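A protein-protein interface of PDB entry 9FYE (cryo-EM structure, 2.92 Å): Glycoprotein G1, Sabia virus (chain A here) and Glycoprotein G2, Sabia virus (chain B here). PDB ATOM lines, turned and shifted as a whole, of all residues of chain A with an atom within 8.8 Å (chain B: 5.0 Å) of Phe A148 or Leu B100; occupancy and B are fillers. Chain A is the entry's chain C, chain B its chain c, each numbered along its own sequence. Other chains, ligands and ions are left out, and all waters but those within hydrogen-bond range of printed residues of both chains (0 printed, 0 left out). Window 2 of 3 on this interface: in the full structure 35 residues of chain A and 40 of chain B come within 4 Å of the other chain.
The guanidinium group of Arg A145 is in hydrogen-bond range of the backbone carbonyl oxygen of Glu B98 (2.6 Å).
NE of Arg A145 is in hydrogen-bond range of O of Leu B99 (3.3 Å).
Gly A139 touches Leu B99.
Gly A143 touches Leu B99 (O to CD2, 3.4 Å).
O of Ser A144 touches CD2 of Leu B99, at 3.1 Å.
Asn B101 touches Arg A145 (OD1 to NH2, 3.5 Å).
CB of Leu B99 touches CE1 of Phe A148, 3.8 Å away.
Phe A148 touches Leu B100.
Phe A148 touches just these residues of chain B: Leu B99 and Leu B100.
Of the printed residues of chain B, Gly A139 touches Leu B99.
Printed residues of chain A within 4 Å of Leu B99: Gly A139, Gly A143, Ser A144, Arg A145 and Phe A148.
Of the printed residues of chain B, Ser A144 touches Leu B99 (3.1 Å).
Printed residues of chain A within 4 Å of Glu B98: Arg A145.
The nearest printed residue of chain B that does not touch Phe A148 is Leu B96 (5.8 Å).
Of the 14 printed residues of chain A, 5 touch a printed residue of chain B.
Printed residues of chain A that touch a printed residue of chain B: Gly A139, Gly A143, Ser A144, Arg A145 and Phe A148.
Hydrophobic or aromatic side chains of chain A that line the printed part of chain B: Phe A148.
Of the 7 printed residues of chain B, 4 touch a printed residue of chain A.
Printed residues of chain B that touch a printed residue of chain A: Glu B98, Leu B99, Leu B100 and Asn B101.
Hydrophobic or aromatic side chains of chain B within 4 Å of the printed part of chain A: Leu B99 and Leu B100.
Among the printed residues, 8 pairs touch across the chains.
Among the printed residues, no Asp or Glu carboxylate lies within 4 Å of a Lys or Arg side-chain nitrogen of the other chain.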
ATOM      1  N   HIS A  31      -0.130  21.707  -2.083  1.00  0.00           N
ATOM      2  CA  HIS A  31       1.211  21.648  -1.509  1.00  0.00           C
ATOM      3  C   HIS A  31       2.212  22.548  -2.226  1.00  0.00           C
ATOM      4  O   HIS A  31       3.325  22.727  -1.721  1.00  0.00           O
ATOM      5  CB  HIS A  31       1.708  20.198  -1.485  1.00  0.00           C
ATOM      6  CG  HIS A  31       1.887  19.589  -2.840  1.00  0.00           C
ATOM      7  ND1 HIS A  31       3.113  19.516  -3.467  1.00  0.00           N
ATOM      8  CD2 HIS A  31       0.998  19.017  -3.685  1.00  0.00           C
ATOM      9  CE1 HIS A  31       2.969  18.929  -4.642  1.00  0.00           C
ATOM     10  NE2 HIS A  31       1.695  18.617  -4.799  1.00  0.00           N
ATOM     11  N   ASP A 132      16.568  21.604   1.291  1.00  0.00           N
ATOM     12  CA  ASP A 132      15.887  20.968   2.412  1.00  0.00           C
ATOM     13  C   ASP A 132      15.374  22.030   3.371  1.00  0.00           C
ATOM     14  O   ASP A 132      14.224  21.972   3.823  1.00  0.00           O
ATOM     15  CB  ASP A 132      16.826  19.994   3.123  1.00  0.00           C
ATOM     16  CG  ASP A 132      17.253  18.842   2.234  1.00  0.00           C
ATOM     17  OD1 ASP A 132      16.964  18.885   1.020  1.00  0.00           O
ATOM     18  OD2 ASP A 132      17.874  17.890   2.749  1.00  0.00           O
ATOM     19  N   LEU A 135      12.388  23.986   1.833  1.00  0.00           N
ATOM     20  CA  LEU A 135      11.153  23.209   1.760  1.00  0.00           C
ATOM     21  C   LEU A 135      10.562  22.988   3.147  1.00  0.00           C
ATOM     22  O   LEU A 135       9.338  23.051   3.327  1.00  0.00           O
ATOM     23  CB  LEU A 135      11.408  21.879   1.054  1.00  0.00           C
ATOM     24  CG  LEU A 135      11.682  21.972  -0.448  1.00  0.00           C
ATOM     25  CD1 LEU A 135      11.723  20.591  -1.072  1.00  0.00           C
ATOM     26  CD2 LEU A 135      10.652  22.842  -1.143  1.00  0.00           C
ATOM     27  N   GLN A 136      11.413  22.723   4.141  1.00  0.00           N
ATOM     28  CA  GLN A 136      10.923  22.573   5.506  1.00  0.00           C
ATOM     29  C   GLN A 136      10.319  23.877   6.010  1.00  0.00           C
ATOM     30  O   GLN A 136       9.303  23.866   6.712  1.00  0.00           O
ATOM     31  CB  GLN A 136      12.055  22.108   6.421  1.00  0.00           C
ATOM     32  CG  GLN A 136      12.493  20.672   6.180  1.00  0.00           C
ATOM     33  CD  GLN A 136      13.812  20.337   6.851  1.00  0.00           C
ATOM     34  OE1 GLN A 136      14.158  20.906   7.885  1.00  0.00           O
ATOM     35  NE2 GLN A 136      14.557  19.413   6.260  1.00  0.00           N
ATOM     36  N   GLY A 139       6.895  24.194   4.561  1.00  0.00           N
ATOM     37  CA  GLY A 139       5.944  23.394   5.316  1.00  0.00           C
ATOM     38  C   GLY A 139       5.590  24.009   6.660  1.00  0.00           C
ATOM     39  O   GLY A 139       4.431  23.984   7.080  1.00  0.00           O
ATOM     40  N   VAL A 140       6.589  24.551   7.355  1.00  0.00           N
ATOM     41  CA  VAL A 140       6.389  25.203   8.647  1.00  0.00           C
ATOM     42  C   VAL A 140       5.540  26.464   8.509  1.00  0.00           C
ATOM     43  O   VAL A 140       4.761  26.809   9.401  1.00  0.00           O
ATOM     44  CB  VAL A 140       7.752  25.494   9.300  1.00  0.00           C
ATOM     45  CG1 VAL A 140       7.620  26.516  10.414  1.00  0.00           C
ATOM     46  CG2 VAL A 140       8.363  24.210   9.826  1.00  0.00           C
ATOM     47  N   GLY A 143       1.995  25.017   6.128  1.00  0.00           N
ATOM     48  CA  GLY A 143       1.340  23.758   6.420  1.00  0.00           C
ATOM     49  C   GLY A 143       1.523  22.676   5.383  1.00  0.00           C
ATOM     50  O   GLY A 143       0.851  21.645   5.466  1.00  0.00           O
ATOM     51  N   SER A 144       2.401  22.879   4.408  1.00  0.00           N
ATOM     52  CA  SER A 144       2.594  21.940   3.320  1.00  0.00           C
ATOM     53  C   SER A 144       3.414  20.731   3.753  1.00  0.00           C
ATOM     54  O   SER A 144       4.220  20.786   4.685  1.00  0.00           O
ATOM     55  CB  SER A 144       3.308  22.620   2.161  1.00  0.00           C
ATOM     56  OG  SER A 144       2.792  23.915   1.973  1.00  0.00           O
ATOM     57  N   ARG A 145       3.216  19.629   3.035  1.00  0.00           N
ATOM     58  CA  ARG A 145       4.029  18.431   3.179  1.00  0.00           C
ATOM     59  C   ARG A 145       4.926  18.237   1.961  1.00  0.00           C
ATOM     60  O   ARG A 145       5.229  17.107   1.573  1.00  0.00           O
ATOM     61  CB  ARG A 145       3.151  17.204   3.413  1.00  0.00           C
ATOM     62  CG  ARG A 145       2.527  17.147   4.796  1.00  0.00           C
ATOM     63  CD  ARG A 145       1.345  16.197   4.839  1.00  0.00           C
ATOM     64  NE  ARG A 145       0.621  16.291   6.100  1.00  0.00           N
ATOM     65  CZ  ARG A 145      -0.427  17.074   6.309  1.00  0.00           C
ATOM     66  NH1 ARG A 145      -0.903  17.857   5.357  1.00  0.00           N
ATOM     67  NH2 ARG A 145      -1.009  17.073   7.505  1.00  0.00           N
ATOM     68  N   ILE A 146       5.340  19.345   1.341  1.00  0.00           N
ATOM     69  CA  ILE A 146       6.195  19.280   0.161  1.00  0.00           C
ATOM     70  C   ILE A 146       7.551  18.676   0.506  1.00  0.00           C
ATOM     71  O   ILE A 146       8.148  17.957  -0.304  1.00  0.00           O
ATOM     72  CB  ILE A 146       6.318  20.675  -0.491  1.00  0.00           C
ATOM     73  CG1 ILE A 146       6.569  20.542  -1.995  1.00  0.00           C
ATOM     74  CG2 ILE A 146       7.384  21.533   0.179  1.00  0.00           C
ATOM     75  CD1 ILE A 146       6.425  21.835  -2.753  1.00  0.00           C
ATOM     76  N   ALA A 147       8.069  18.970   1.702  1.00  0.00           N
ATOM     77  CA  ALA A 147       9.368  18.434   2.095  1.00  0.00           C
ATOM     78  C   ALA A 147       9.324  16.917   2.216  1.00  0.00           C
ATOM     79  O   ALA A 147      10.267  16.226   1.815  1.00  0.00           O
ATOM     80  CB  ALA A 147       9.823  19.066   3.408  1.00  0.00           C
ATOM     81  N   PHE A 148       8.238  16.382   2.773  1.00  0.00           N
ATOM     82  CA  PHE A 148       8.098  14.936   2.892  1.00  0.00           C
ATOM     83  C   PHE A 148       7.868  14.276   1.540  1.00  0.00           C
ATOM     84  O   PHE A 148       8.298  13.137   1.330  1.00  0.00           O
ATOM     85  CB  PHE A 148       6.959  14.594   3.853  1.00  0.00           C
ATOM     86  CG  PHE A 148       7.157  15.130   5.242  1.00  0.00           C
ATOM     87  CD1 PHE A 148       6.890  16.455   5.536  1.00  0.00           C
ATOM     88  CD2 PHE A 148       7.616  14.307   6.253  1.00  0.00           C
ATOM     89  CE1 PHE A 148       7.074  16.948   6.808  1.00  0.00           C
ATOM     90  CE2 PHE A 148       7.802  14.796   7.529  1.00  0.00           C
ATOM     91  CZ  PHE A 148       7.530  16.118   7.807  1.00  0.00           C
ATOM     92  N   SER A 149       7.193  14.961   0.623  1.00  0.00           N
ATOM     93  CA  SER A 149       6.988  14.420  -0.712  1.00  0.00           C
ATOM     94  C   SER A 149       8.313  14.328  -1.459  1.00  0.00           C
ATOM     95  O   SER A 149       9.170  15.210  -1.348  1.00  0.00           O
ATOM     96  CB  SER A 149       6.000  15.285  -1.493  1.00  0.00           C
ATOM     97  OG  SER A 149       6.576  16.531  -1.843  1.00  0.00           O
ATOM     98  N   ASN A 150       8.482  13.239  -2.205  1.00  0.00           N
ATOM     99  CA  ASN A 150       9.696  12.992  -2.980  1.00  0.00           C
ATOM    100  C   ASN A 150      10.051  14.164  -3.891  1.00  0.00           C
ATOM    101  O   ASN A 150      11.015  14.100  -4.654  1.00  0.00           O
ATOM    102  CB  ASN A 150       9.541  11.717  -3.811  1.00  0.00           C
ATOM    103  CG  ASN A 150       9.385  10.478  -2.952  1.00  0.00           C
ATOM    104  OD1 ASN A 150       8.338   9.830  -2.962  1.00  0.00           O
ATOM    105  ND2 ASN A 150      10.428  10.142  -2.204  1.00  0.00           N
ATOM    106  N   LEU B  96       4.467  20.777  13.554  1.00  0.00           N
ATOM    107  CA  LEU B  96       5.217  19.573  13.205  1.00  0.00           C
ATOM    108  C   LEU B  96       4.383  18.312  13.406  1.00  0.00           C
ATOM    109  O   LEU B  96       4.515  17.350  12.642  1.00  0.00           O
ATOM    110  CB  LEU B  96       6.524  19.498  13.995  1.00  0.00           C
ATOM    111  CG  LEU B  96       7.753  20.263  13.486  1.00  0.00           C
ATOM    112  CD1 LEU B  96       7.551  21.752  13.349  1.00  0.00           C
ATOM    113  CD2 LEU B  96       8.906  19.995  14.426  1.00  0.00           C
ATOM    114  N   LYS B  97       3.525  18.287  14.427  1.00  0.00           N
ATOM    115  CA  LYS B  97       2.552  17.204  14.525  1.00  0.00           C
ATOM    116  C   LYS B  97       1.612  17.195  13.325  1.00  0.00           C
ATOM    117  O   LYS B  97       1.239  16.129  12.827  1.00  0.00           O
ATOM    118  CB  LYS B  97       1.748  17.320  15.817  1.00  0.00           C
ATOM    119  CG  LYS B  97       2.548  17.150  17.078  1.00  0.00           C
ATOM    120  CD  LYS B  97       1.621  17.049  18.263  1.00  0.00           C
ATOM    121  CE  LYS B  97       2.382  16.999  19.562  1.00  0.00           C
ATOM    122  NZ  LYS B  97       1.451  16.942  20.717  1.00  0.00           N
ATOM    123  N   GLU B  98       1.199  18.379  12.868  1.00  0.00           N
ATOM    124  CA  GLU B  98       0.306  18.471  11.715  1.00  0.00           C
ATOM    125  C   GLU B  98       0.941  17.875  10.466  1.00  0.00           C
ATOM    126  O   GLU B  98       0.304  17.109   9.734  1.00  0.00           O
ATOM    127  CB  GLU B  98      -0.085  19.925  11.465  1.00  0.00           C
ATOM    128  CG  GLU B  98      -0.722  20.156  10.105  1.00  0.00           C
ATOM    129  CD  GLU B  98      -1.112  21.597   9.873  1.00  0.00           C
ATOM    130  OE1 GLU B  98      -0.663  22.470  10.641  1.00  0.00           O
ATOM    131  OE2 GLU B  98      -1.865  21.857   8.914  1.00  0.00           O
ATOM    132  N   LEU B  99       2.198  18.231  10.197  1.00  0.00           N
ATOM    133  CA  LEU B  99       2.871  17.787   8.982  1.00  0.00           C
ATOM    134  C   LEU B  99       3.127  16.288   8.971  1.00  0.00           C
ATOM    135  O   LEU B  99       3.331  15.714   7.896  1.00  0.00           O
ATOM    136  CB  LEU B  99       4.197  18.527   8.815  1.00  0.00           C
ATOM    137  CG  LEU B  99       4.123  20.051   8.782  1.00  0.00           C
ATOM    138  CD1 LEU B  99       5.514  20.653   8.692  1.00  0.00           C
ATOM    139  CD2 LEU B  99       3.252  20.517   7.639  1.00  0.00           C
ATOM    140  N   LEU B 100       3.125  15.647  10.135  1.00  0.00           N
ATOM    141  CA  LEU B 100       3.405  14.226  10.256  1.00  0.00           C
ATOM    142  C   LEU B 100       2.143  13.377  10.325  1.00  0.00           C
ATOM    143  O   LEU B 100       2.233  12.179  10.605  1.00  0.00           O
ATOM    144  CB  LEU B 100       4.274  13.972  11.485  1.00  0.00           C
ATOM    145  CG  LEU B 100       5.757  14.260  11.264  1.00  0.00           C
ATOM    146  CD1 LEU B 100       6.479  14.328  12.589  1.00  0.00           C
ATOM    147  CD2 LEU B 100       6.376  13.219  10.354  1.00  0.00           C
ATOM    148  N   ASN B 101       0.974  13.973  10.085  1.00  0.00           N
ATOM    149  CA  ASN B 101      -0.307  13.267  10.140  1.00  0.00           C
ATOM    150  C   ASN B 101      -0.547  12.653  11.517  1.00  0.00           C
ATOM    151  O   ASN B 101      -1.063  11.541  11.644  1.00  0.00           O
ATOM    152  CB  ASN B 101      -0.404  12.207   9.041  1.00  0.00           C
ATOM    153  CG  ASN B 101      -0.659  12.810   7.681  1.00  0.00           C
ATOM    154  OD1 ASN B 101      -1.578  13.608   7.510  1.00  0.00           O
ATOM    155  ND2 ASN B 101       0.159  12.437   6.705  1.00  0.00           N
ATOM    156  N   THR B 102      -0.176  13.392  12.548  1.00  0.00           N
ATOM    157  CA  THR B 102      -0.357  13.126  13.961  1.00  0.00           C
ATOM    158  C   THR B 102      -1.374  14.112  14.525  1.00  0.00           C
ATOM    159  O   THR B 102      -1.450  15.250  14.053  1.00  0.00           O
ATOM    160  CB  THR B 102       0.986  13.269  14.695  1.00  0.00           C
ATOM    161  OG1 THR B 102       1.921  12.315  14.174  1.00  0.00           O
ATOM    162  CG2 THR B 102       0.853  13.059  16.194  1.00  0.00           C
